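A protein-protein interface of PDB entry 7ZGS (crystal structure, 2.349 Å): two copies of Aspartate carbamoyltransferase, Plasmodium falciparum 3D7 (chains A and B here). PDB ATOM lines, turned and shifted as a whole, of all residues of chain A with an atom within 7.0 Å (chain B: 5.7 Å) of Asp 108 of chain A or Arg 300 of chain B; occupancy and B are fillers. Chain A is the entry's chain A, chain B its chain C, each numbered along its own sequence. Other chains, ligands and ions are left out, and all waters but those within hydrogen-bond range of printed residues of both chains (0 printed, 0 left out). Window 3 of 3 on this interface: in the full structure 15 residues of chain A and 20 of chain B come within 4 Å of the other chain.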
ATOM      1  N   GLY A 103     -27.907  26.426  30.950  1.00  0.00           N
ATOM      2  CA  GLY A 103     -28.444  25.047  30.894  1.00  0.00           C
ATOM      3  C   GLY A 103     -27.716  24.083  29.945  1.00  0.00           C
ATOM      4  O   GLY A 103     -28.230  22.973  29.813  1.00  0.00           O
ATOM      5  N   GLU A 104     -26.634  24.492  29.250  1.00  0.00           N
ATOM      6  CA  GLU A 104     -25.795  23.655  28.341  1.00  0.00           C
ATOM      7  C   GLU A 104     -24.658  22.978  29.130  1.00  0.00           C
ATOM      8  O   GLU A 104     -24.177  23.579  30.096  1.00  0.00           O
ATOM      9  CB  GLU A 104     -25.178  24.520  27.234  1.00  0.00           C
ATOM     10  CG  GLU A 104     -24.258  23.763  26.280  1.00  0.00           C
ATOM     11  CD  GLU A 104     -23.485  24.605  25.281  1.00  0.00           C
ATOM     12  OE1 GLU A 104     -23.240  25.823  25.548  1.00  0.00           O
ATOM     13  OE2 GLU A 104     -23.133  24.029  24.224  1.00  0.00           O
ATOM     14  N   THR A 105     -24.232  21.780  28.713  1.00  0.00           N
ATOM     15  CA  THR A 105     -23.224  20.949  29.422  1.00  0.00           C
ATOM     16  C   THR A 105     -21.838  21.580  29.271  1.00  0.00           C
ATOM     17  O   THR A 105     -21.521  22.193  28.240  1.00  0.00           O
ATOM     18  CB  THR A 105     -23.177  19.486  28.946  1.00  0.00           C
ATOM     19  OG1 THR A 105     -22.757  19.411  27.574  1.00  0.00           O
ATOM     20  CG2 THR A 105     -24.477  18.728  29.145  1.00  0.00           C
ATOM     21  N   VAL A 106     -21.016  21.404  30.287  1.00  0.00           N
ATOM     22  CA  VAL A 106     -19.591  21.805  30.252  1.00  0.00           C
ATOM     23  C   VAL A 106     -18.948  21.042  29.092  1.00  0.00           C
ATOM     24  O   VAL A 106     -18.199  21.648  28.329  1.00  0.00           O
ATOM     25  CB  VAL A 106     -18.923  21.574  31.620  1.00  0.00           C
ATOM     26  CG1 VAL A 106     -17.459  22.039  31.628  1.00  0.00           C
ATOM     27  CG2 VAL A 106     -19.683  22.313  32.716  1.00  0.00           C
ATOM     28  N   GLU A 107     -19.295  19.779  28.912  1.00  0.00           N
ATOM     29  CA  GLU A 107     -18.703  18.884  27.880  1.00  0.00           C
ATOM     30  C   GLU A 107     -18.876  19.516  26.504  1.00  0.00           C
ATOM     31  O   GLU A 107     -17.845  19.698  25.811  1.00  0.00           O
ATOM     32  CB  GLU A 107     -19.327  17.489  27.954  1.00  0.00           C
ATOM     33  CG  GLU A 107     -18.873  16.701  29.181  1.00  0.00           C
ATOM     34  CD  GLU A 107     -19.768  16.732  30.431  1.00  0.00           C
ATOM     35  OE1 GLU A 107     -20.613  17.694  30.552  1.00  0.00           O
ATOM     36  OE2 GLU A 107     -19.579  15.794  31.333  1.00  0.00           O
ATOM     37  N   ASP A 108     -20.122  19.851  26.150  1.00  0.00           N
ATOM     38  CA  ASP A 108     -20.487  20.470  24.848  1.00  0.00           C
ATOM     39  C   ASP A 108     -19.743  21.788  24.724  1.00  0.00           C
ATOM     40  O   ASP A 108     -19.105  22.001  23.668  1.00  0.00           O
ATOM     41  CB  ASP A 108     -22.001  20.650  24.694  1.00  0.00           C
ATOM     42  CG  ASP A 108     -22.731  19.330  24.505  1.00  0.00           C
ATOM     43  OD1 ASP A 108     -22.024  18.275  24.438  1.00  0.00           O
ATOM     44  OD2 ASP A 108     -24.011  19.375  24.414  1.00  0.00           O
ATOM     45  N   ALA A 109     -19.780  22.609  25.773  1.00  0.00           N
ATOM     46  CA  ALA A 109     -19.205  23.975  25.762  1.00  0.00           C
ATOM     47  C   ALA A 109     -17.718  23.899  25.389  1.00  0.00           C
ATOM     48  O   ALA A 109     -17.282  24.661  24.477  1.00  0.00           O
ATOM     49  CB  ALA A 109     -19.429  24.689  27.077  1.00  0.00           C
ATOM     50  N   PHE A 110     -16.963  23.007  26.028  1.00  0.00           N
ATOM     51  CA  PHE A 110     -15.489  22.986  25.859  1.00  0.00           C
ATOM     52  C   PHE A 110     -15.150  22.224  24.584  1.00  0.00           C
ATOM     53  O   PHE A 110     -14.109  22.564  23.961  1.00  0.00           O
ATOM     54  CB  PHE A 110     -14.780  22.472  27.109  1.00  0.00           C
ATOM     55  CG  PHE A 110     -14.397  23.606  28.019  1.00  0.00           C
ATOM     56  CD1 PHE A 110     -13.141  24.175  27.939  1.00  0.00           C
ATOM     57  CD2 PHE A 110     -15.333  24.174  28.861  1.00  0.00           C
ATOM     58  CE1 PHE A 110     -12.812  25.262  28.733  1.00  0.00           C
ATOM     59  CE2 PHE A 110     -14.993  25.242  29.668  1.00  0.00           C
ATOM     60  CZ  PHE A 110     -13.733  25.780  29.602  1.00  0.00           C
ATOM     61  N   LYS A 111     -16.012  21.291  24.171  1.00  0.00           N
ATOM     62  CA  LYS A 111     -15.832  20.547  22.902  1.00  0.00           C
ATOM     63  C   LYS A 111     -15.939  21.563  21.763  1.00  0.00           C
ATOM     64  O   LYS A 111     -15.125  21.523  20.845  1.00  0.00           O
ATOM     65  CB  LYS A 111     -16.839  19.391  22.823  1.00  0.00           C
ATOM     66  CG  LYS A 111     -16.582  18.397  21.698  1.00  0.00           C
ATOM     67  CD  LYS A 111     -17.289  17.056  21.843  1.00  0.00           C
ATOM     68  CE  LYS A 111     -16.758  16.059  20.822  1.00  0.00           C
ATOM     69  NZ  LYS A 111     -15.282  15.865  20.955  1.00  0.00           N
ATOM     70  N   ILE A 112     -16.859  22.503  21.859  1.00  0.00           N
ATOM     71  CA  ILE A 112     -17.014  23.560  20.809  1.00  0.00           C
ATOM     72  C   ILE A 112     -15.884  24.605  20.892  1.00  0.00           C
ATOM     73  O   ILE A 112     -15.266  24.879  19.877  1.00  0.00           O
ATOM     74  CB  ILE A 112     -18.373  24.251  20.931  1.00  0.00           C
ATOM     75  CG1 ILE A 112     -19.498  23.260  20.687  1.00  0.00           C
ATOM     76  CG2 ILE A 112     -18.423  25.442  20.000  1.00  0.00           C
ATOM     77  CD1 ILE A 112     -20.815  23.694  21.288  1.00  0.00           C
ATOM     78  N   LEU A 113     -15.704  25.237  22.043  1.00  0.00           N
ATOM     79  CA  LEU A 113     -14.826  26.421  22.171  1.00  0.00           C
ATOM     80  C   LEU A 113     -13.408  26.016  21.780  1.00  0.00           C
ATOM     81  O   LEU A 113     -12.742  26.783  21.073  1.00  0.00           O
ATOM     82  CB  LEU A 113     -14.912  26.890  23.615  1.00  0.00           C
ATOM     83  CG  LEU A 113     -14.017  28.063  23.992  1.00  0.00           C
ATOM     84  CD1 LEU A 113     -14.286  29.296  23.115  1.00  0.00           C
ATOM     85  CD2 LEU A 113     -14.231  28.373  25.475  1.00  0.00           C
ATOM     86  N   SER A 114     -13.004  24.818  22.209  1.00  0.00           N
ATOM     87  CA  SER A 114     -11.664  24.240  21.944  1.00  0.00           C
ATOM     88  C   SER A 114     -11.438  24.051  20.442  1.00  0.00           C
ATOM     89  O   SER A 114     -10.273  23.997  20.087  1.00  0.00           O
ATOM     90  CB  SER A 114     -11.360  22.992  22.751  1.00  0.00           C
ATOM     91  OG  SER A 114     -12.025  21.832  22.298  1.00  0.00           O
ATOM     92  N   ILE A 132     -13.907  18.452  34.021  1.00  0.00           N
ATOM     93  CA  ILE A 132     -14.790  18.143  32.859  1.00  0.00           C
ATOM     94  C   ILE A 132     -14.232  18.853  31.623  1.00  0.00           C
ATOM     95  O   ILE A 132     -14.161  18.198  30.543  1.00  0.00           O
ATOM     96  CB  ILE A 132     -16.250  18.530  33.128  1.00  0.00           C
ATOM     97  CG1 ILE A 132     -16.881  17.680  34.230  1.00  0.00           C
ATOM     98  CG2 ILE A 132     -17.062  18.463  31.828  1.00  0.00           C
ATOM     99  CD1 ILE A 132     -18.139  18.274  34.811  1.00  0.00           C
ATOM    100  N   SER A 136     -13.033  17.093  28.030  1.00  0.00           N
ATOM    101  CA  SER A 136     -13.893  17.376  26.851  1.00  0.00           C
ATOM    102  C   SER A 136     -13.181  18.273  25.811  1.00  0.00           C
ATOM    103  O   SER A 136     -13.677  18.351  24.656  1.00  0.00           O
ATOM    104  CB  SER A 136     -15.222  17.951  27.308  1.00  0.00           C
ATOM    105  OG  SER A 136     -16.309  17.324  26.616  1.00  0.00           O
ATOM    106  N   HIS B 296     -26.992  19.700  14.083  1.00  0.00           N
ATOM    107  CA  HIS B 296     -27.697  20.453  15.147  1.00  0.00           C
ATOM    108  C   HIS B 296     -26.932  21.770  15.319  1.00  0.00           C
ATOM    109  O   HIS B 296     -25.710  21.750  15.484  1.00  0.00           O
ATOM    110  CB  HIS B 296     -27.793  19.638  16.424  1.00  0.00           C
ATOM    111  CG  HIS B 296     -28.712  20.199  17.457  1.00  0.00           C
ATOM    112  ND1 HIS B 296     -28.708  21.522  17.810  1.00  0.00           N
ATOM    113  CD2 HIS B 296     -29.644  19.610  18.240  1.00  0.00           C
ATOM    114  CE1 HIS B 296     -29.605  21.738  18.757  1.00  0.00           C
ATOM    115  NE2 HIS B 296     -30.211  20.577  19.029  1.00  0.00           N
ATOM    116  N   LEU B 298     -26.883  23.730  17.710  1.00  0.00           N
ATOM    117  CA  LEU B 298     -26.437  23.689  19.144  1.00  0.00           C
ATOM    118  C   LEU B 298     -26.765  25.026  19.801  1.00  0.00           C
ATOM    119  O   LEU B 298     -26.930  26.012  19.089  1.00  0.00           O
ATOM    120  CB  LEU B 298     -24.946  23.335  19.203  1.00  0.00           C
ATOM    121  CG  LEU B 298     -24.618  21.905  18.752  1.00  0.00           C
ATOM    122  CD1 LEU B 298     -23.119  21.615  18.841  1.00  0.00           C
ATOM    123  CD2 LEU B 298     -25.389  20.850  19.568  1.00  0.00           C
ATOM    124  N   PRO B 299     -26.984  25.123  21.128  1.00  0.00           N
ATOM    125  CA  PRO B 299     -26.807  24.027  22.065  1.00  0.00           C
ATOM    126  C   PRO B 299     -27.996  23.073  22.066  1.00  0.00           C
ATOM    127  O   PRO B 299     -29.102  23.533  21.907  1.00  0.00           O
ATOM    128  CB  PRO B 299     -26.730  24.727  23.438  1.00  0.00           C
ATOM    129  CG  PRO B 299     -27.526  25.993  23.266  1.00  0.00           C
ATOM    130  CD  PRO B 299     -27.443  26.350  21.800  1.00  0.00           C
ATOM    131  N   ARG B 300     -27.732  21.782  22.264  1.00  0.00           N
ATOM    132  CA  ARG B 300     -28.747  20.718  22.454  1.00  0.00           C
ATOM    133  C   ARG B 300     -29.130  20.684  23.935  1.00  0.00           C
ATOM    134  O   ARG B 300     -28.361  21.203  24.763  1.00  0.00           O
ATOM    135  CB  ARG B 300     -28.150  19.387  22.012  1.00  0.00           C
ATOM    136  CG  ARG B 300     -26.998  18.913  22.900  1.00  0.00           C
ATOM    137  CD  ARG B 300     -26.728  17.428  22.758  1.00  0.00           C
ATOM    138  NE  ARG B 300     -25.382  17.052  23.171  1.00  0.00           N
ATOM    139  CZ  ARG B 300     -24.797  15.896  22.898  1.00  0.00           C
ATOM    140  NH1 ARG B 300     -25.437  14.948  22.236  1.00  0.00           N
ATOM    141  NH2 ARG B 300     -23.560  15.678  23.304  1.00  0.00           N
ATOM    142  N   VAL B 301     -30.254  20.064  24.255  1.00  0.00           N
ATOM    143  CA  VAL B 301     -30.674  19.687  25.634  1.00  0.00           C
ATOM    144  C   VAL B 301     -30.808  18.164  25.638  1.00  0.00           C
ATOM    145  O   VAL B 301     -29.778  17.510  25.889  1.00  0.00           O
ATOM    146  CB  VAL B 301     -31.971  20.421  26.024  1.00  0.00           C
ATOM    147  CG1 VAL B 301     -32.537  19.943  27.351  1.00  0.00           C
ATOM    148  CG2 VAL B 301     -31.755  21.931  26.029  1.00  0.00           C
ATOM    149  N   ASN B 302     -31.981  17.612  25.309  1.00  0.00           N
ATOM    150  CA  ASN B 302     -32.182  16.136  25.233  1.00  0.00           C
ATOM    151  C   ASN B 302     -32.479  15.701  23.783  1.00  0.00           C
ATOM    152  O   ASN B 302     -32.411  14.496  23.520  1.00  0.00           O
ATOM    153  CB  ASN B 302     -33.245  15.658  26.217  1.00  0.00           C
ATOM    154  CG  ASN B 302     -33.157  14.165  26.478  1.00  0.00           C
ATOM    155  OD1 ASN B 302     -32.316  13.469  25.903  1.00  0.00           O
ATOM    156  ND2 ASN B 302     -34.023  13.650  27.343  1.00  0.00           N
ATOM    157  N   GLU B 303     -32.783  16.623  22.861  1.00  0.00           N
ATOM    158  CA  GLU B 303     -33.098  16.307  21.432  1.00  0.00           C
ATOM    159  C   GLU B 303     -32.165  15.231  20.868  1.00  0.00           C
ATOM    160  O   GLU B 303     -32.578  14.514  19.997  1.00  0.00           O
ATOM    161  CB  GLU B 303     -32.891  17.493  20.475  1.00  0.00           C
ATOM    162  CG  GLU B 303     -33.327  18.858  20.972  1.00  0.00           C
ATOM    163  CD  GLU B 303     -32.191  19.543  21.670  1.00  0.00           C
ATOM    164  OE1 GLU B 303     -31.662  18.873  22.538  1.00  0.00           O
ATOM    165  OE2 GLU B 303     -31.808  20.707  21.317  1.00  0.00           O
ATOM    166  N   ILE B 304     -30.901  15.221  21.268  1.00  0.00           N
ATOM    167  CA  ILE B 304     -29.889  14.202  20.848  1.00  0.00           C
ATOM    168  C   ILE B 304     -29.205  13.660  22.105  1.00  0.00           C
ATOM    169  O   ILE B 304     -28.541  14.439  22.800  1.00  0.00           O
ATOM    170  CB  ILE B 304     -28.858  14.785  19.863  1.00  0.00           C
ATOM    171  CG1 ILE B 304     -29.506  15.598  18.744  1.00  0.00           C
ATOM    172  CG2 ILE B 304     -27.963  13.698  19.303  1.00  0.00           C
ATOM    173  CD1 ILE B 304     -28.574  15.841  17.573  1.00  0.00           C
ATOM    174  N   LYS B 305     -29.373  12.363  22.362  1.00  0.00           N
ATOM    175  CA  LYS B 305     -28.770  11.627  23.512  1.00  0.00           C
ATOM    176  C   LYS B 305     -27.254  11.529  23.285  1.00  0.00           C
ATOM    177  O   LYS B 305     -26.832  11.316  22.117  1.00  0.00           O
ATOM    178  CB  LYS B 305     -29.489  10.275  23.661  1.00  0.00           C
ATOM    179  CG  LYS B 305     -28.835   9.201  24.530  1.00  0.00           C
ATOM    180  CD  LYS B 305     -28.452   9.590  25.959  1.00  0.00           C
ATOM    181  CE  LYS B 305     -27.731   8.483  26.707  1.00  0.00           C
ATOM    182  NZ  LYS B 305     -26.287   8.457  26.374  1.00  0.00           N
ATOM    183  N   VAL B 306     -26.483  11.712  24.361  1.00  0.00           N
ATOM    184  CA  VAL B 306     -24.988  11.700  24.385  1.00  0.00           C
ATOM    185  C   VAL B 306     -24.448  10.441  23.688  1.00  0.00           C
ATOM    186  O   VAL B 306     -23.317  10.475  23.226  1.00  0.00           O
ATOM    187  CB  VAL B 306     -24.496  11.822  25.839  1.00  0.00           C
ATOM    188  CG1 VAL B 306     -22.983  11.694  25.953  1.00  0.00           C
ATOM    189  CG2 VAL B 306     -24.985  13.120  26.469  1.00  0.00           C
ATOM    190  N   ASP B 309     -23.285  10.986  20.071  1.00  0.00           N
ATOM    191  CA  ASP B 309     -22.040  11.804  19.960  1.00  0.00           C
ATOM    192  C   ASP B 309     -20.923  10.802  19.572  1.00  0.00           C
ATOM    193  O   ASP B 309     -20.005  11.158  18.855  1.00  0.00           O
ATOM    194  CB  ASP B 309     -22.036  12.743  21.196  1.00  0.00           C
ATOM    195  CG  ASP B 309     -20.746  13.022  21.953  1.00  0.00           C
ATOM    196  OD1 ASP B 309     -19.797  13.554  21.326  1.00  0.00           O
ATOM    197  OD2 ASP B 309     -20.699  12.756  23.190  1.00  0.00           O
ATOM    198  N   TYR B 316     -22.452  17.155  14.338  1.00  0.00           N
ATOM    199  CA  TYR B 316     -22.871  18.478  14.884  1.00  0.00           C
ATOM    200  C   TYR B 316     -21.673  19.250  15.466  1.00  0.00           C
ATOM    201  O   TYR B 316     -21.679  20.498  15.365  1.00  0.00           O
ATOM    202  CB  TYR B 316     -24.011  18.396  15.916  1.00  0.00           C
ATOM    203  CG  TYR B 316     -24.159  17.113  16.676  1.00  0.00           C
ATOM    204  CD1 TYR B 316     -23.650  16.970  17.951  1.00  0.00           C
ATOM    205  CD2 TYR B 316     -24.842  16.046  16.124  1.00  0.00           C
ATOM    206  CE1 TYR B 316     -23.788  15.785  18.647  1.00  0.00           C
ATOM    207  CE2 TYR B 316     -24.983  14.851  16.801  1.00  0.00           C
ATOM    208  CZ  TYR B 316     -24.448  14.722  18.064  1.00  0.00           C
ATOM    209  OH  TYR B 316     -24.570  13.533  18.706  1.00  0.00           O
ATOM    210  N   PHE B 317     -20.668  18.574  16.039  1.00  0.00           N
ATOM    211  CA  PHE B 317     -19.487  19.270  16.618  1.00  0.00           C
ATOM    212  C   PHE B 317     -18.559  19.720  15.480  1.00  0.00           C
ATOM    213  O   PHE B 317     -18.022  20.840  15.570  1.00  0.00           O
ATOM    214  CB  PHE B 317     -18.778  18.429  17.677  1.00  0.00           C
ATOM    215  CG  PHE B 317     -19.613  18.171  18.902  1.00  0.00           C
ATOM    216  CD1 PHE B 317     -19.949  19.202  19.761  1.00  0.00           C
ATOM    217  CD2 PHE B 317     -20.089  16.903  19.183  1.00  0.00           C
ATOM    218  CE1 PHE B 317     -20.717  18.956  20.890  1.00  0.00           C
ATOM    219  CE2 PHE B 317     -20.850  16.664  20.319  1.00  0.00           C
ATOM    220  CZ  PHE B 317     -21.161  17.689  21.175  1.00  0.00           C
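The side-chain carboxylate of Asp 108 of chain A is in salt-bridge range of the guanidinium group of Arg 300 of chain B (3.0 Å).
NH1 of Arg 300 of chain B lies within hydrogen-bond range of O of Ile 304 of chain B (3.2 Å). OG1 of Thr 105 of chain A sits at hydrogen-bond distance from N of Asp 108 of chain A (3.0 Å). OH of Tyr 316 of chain B lies within hydrogen-bond range of N of Asp 309 of chain B, at 3.2 Å. ND1 of His 296 of chain B sits at hydrogen-bond distance from N of Leu 298 of chain B (2.9 Å). O of Lys 111 of chain A sits at hydrogen-bond distance from OG of Ser 114 of chain A (3.4 Å).
Pro 299 of chain B touches Glu 104 of chain A (CB to CD, 3.7 Å). OD1 of Asp 108 of chain A touches CZ of Phe 317 of chain B (3.4 Å). OD1 of Asp 309 of chain B touches CE of Lys 111 of chain A, 3.97 Å away. Lys 111 of chain A touches Phe 317 of chain B (CE to CD2, 3.8 Å). Ile 112 of chain A touches Leu 298 of chain B.
Asp 108 of chain A touches two residues of chain B. Of the printed residues of chain A, Asp 309 of chain B touches Lys 111 (3.97 Å). Of the printed residues of chain A, Leu 298 of chain B touches Ile 112 (3.95 Å). Asn 302 of chain B touches none of the printed residues of chain A. The nearest printed residue of chain B that does not touch Ile 112 of chain A is Phe 317 of chain B (4.2 Å).
Hydrophobic or aromatic side chains of chain A within 4 Å of the printed part of chain B: Ile 112. Among the printed residues, 6 pairs touch across the chains.
No position is printed for both chains.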
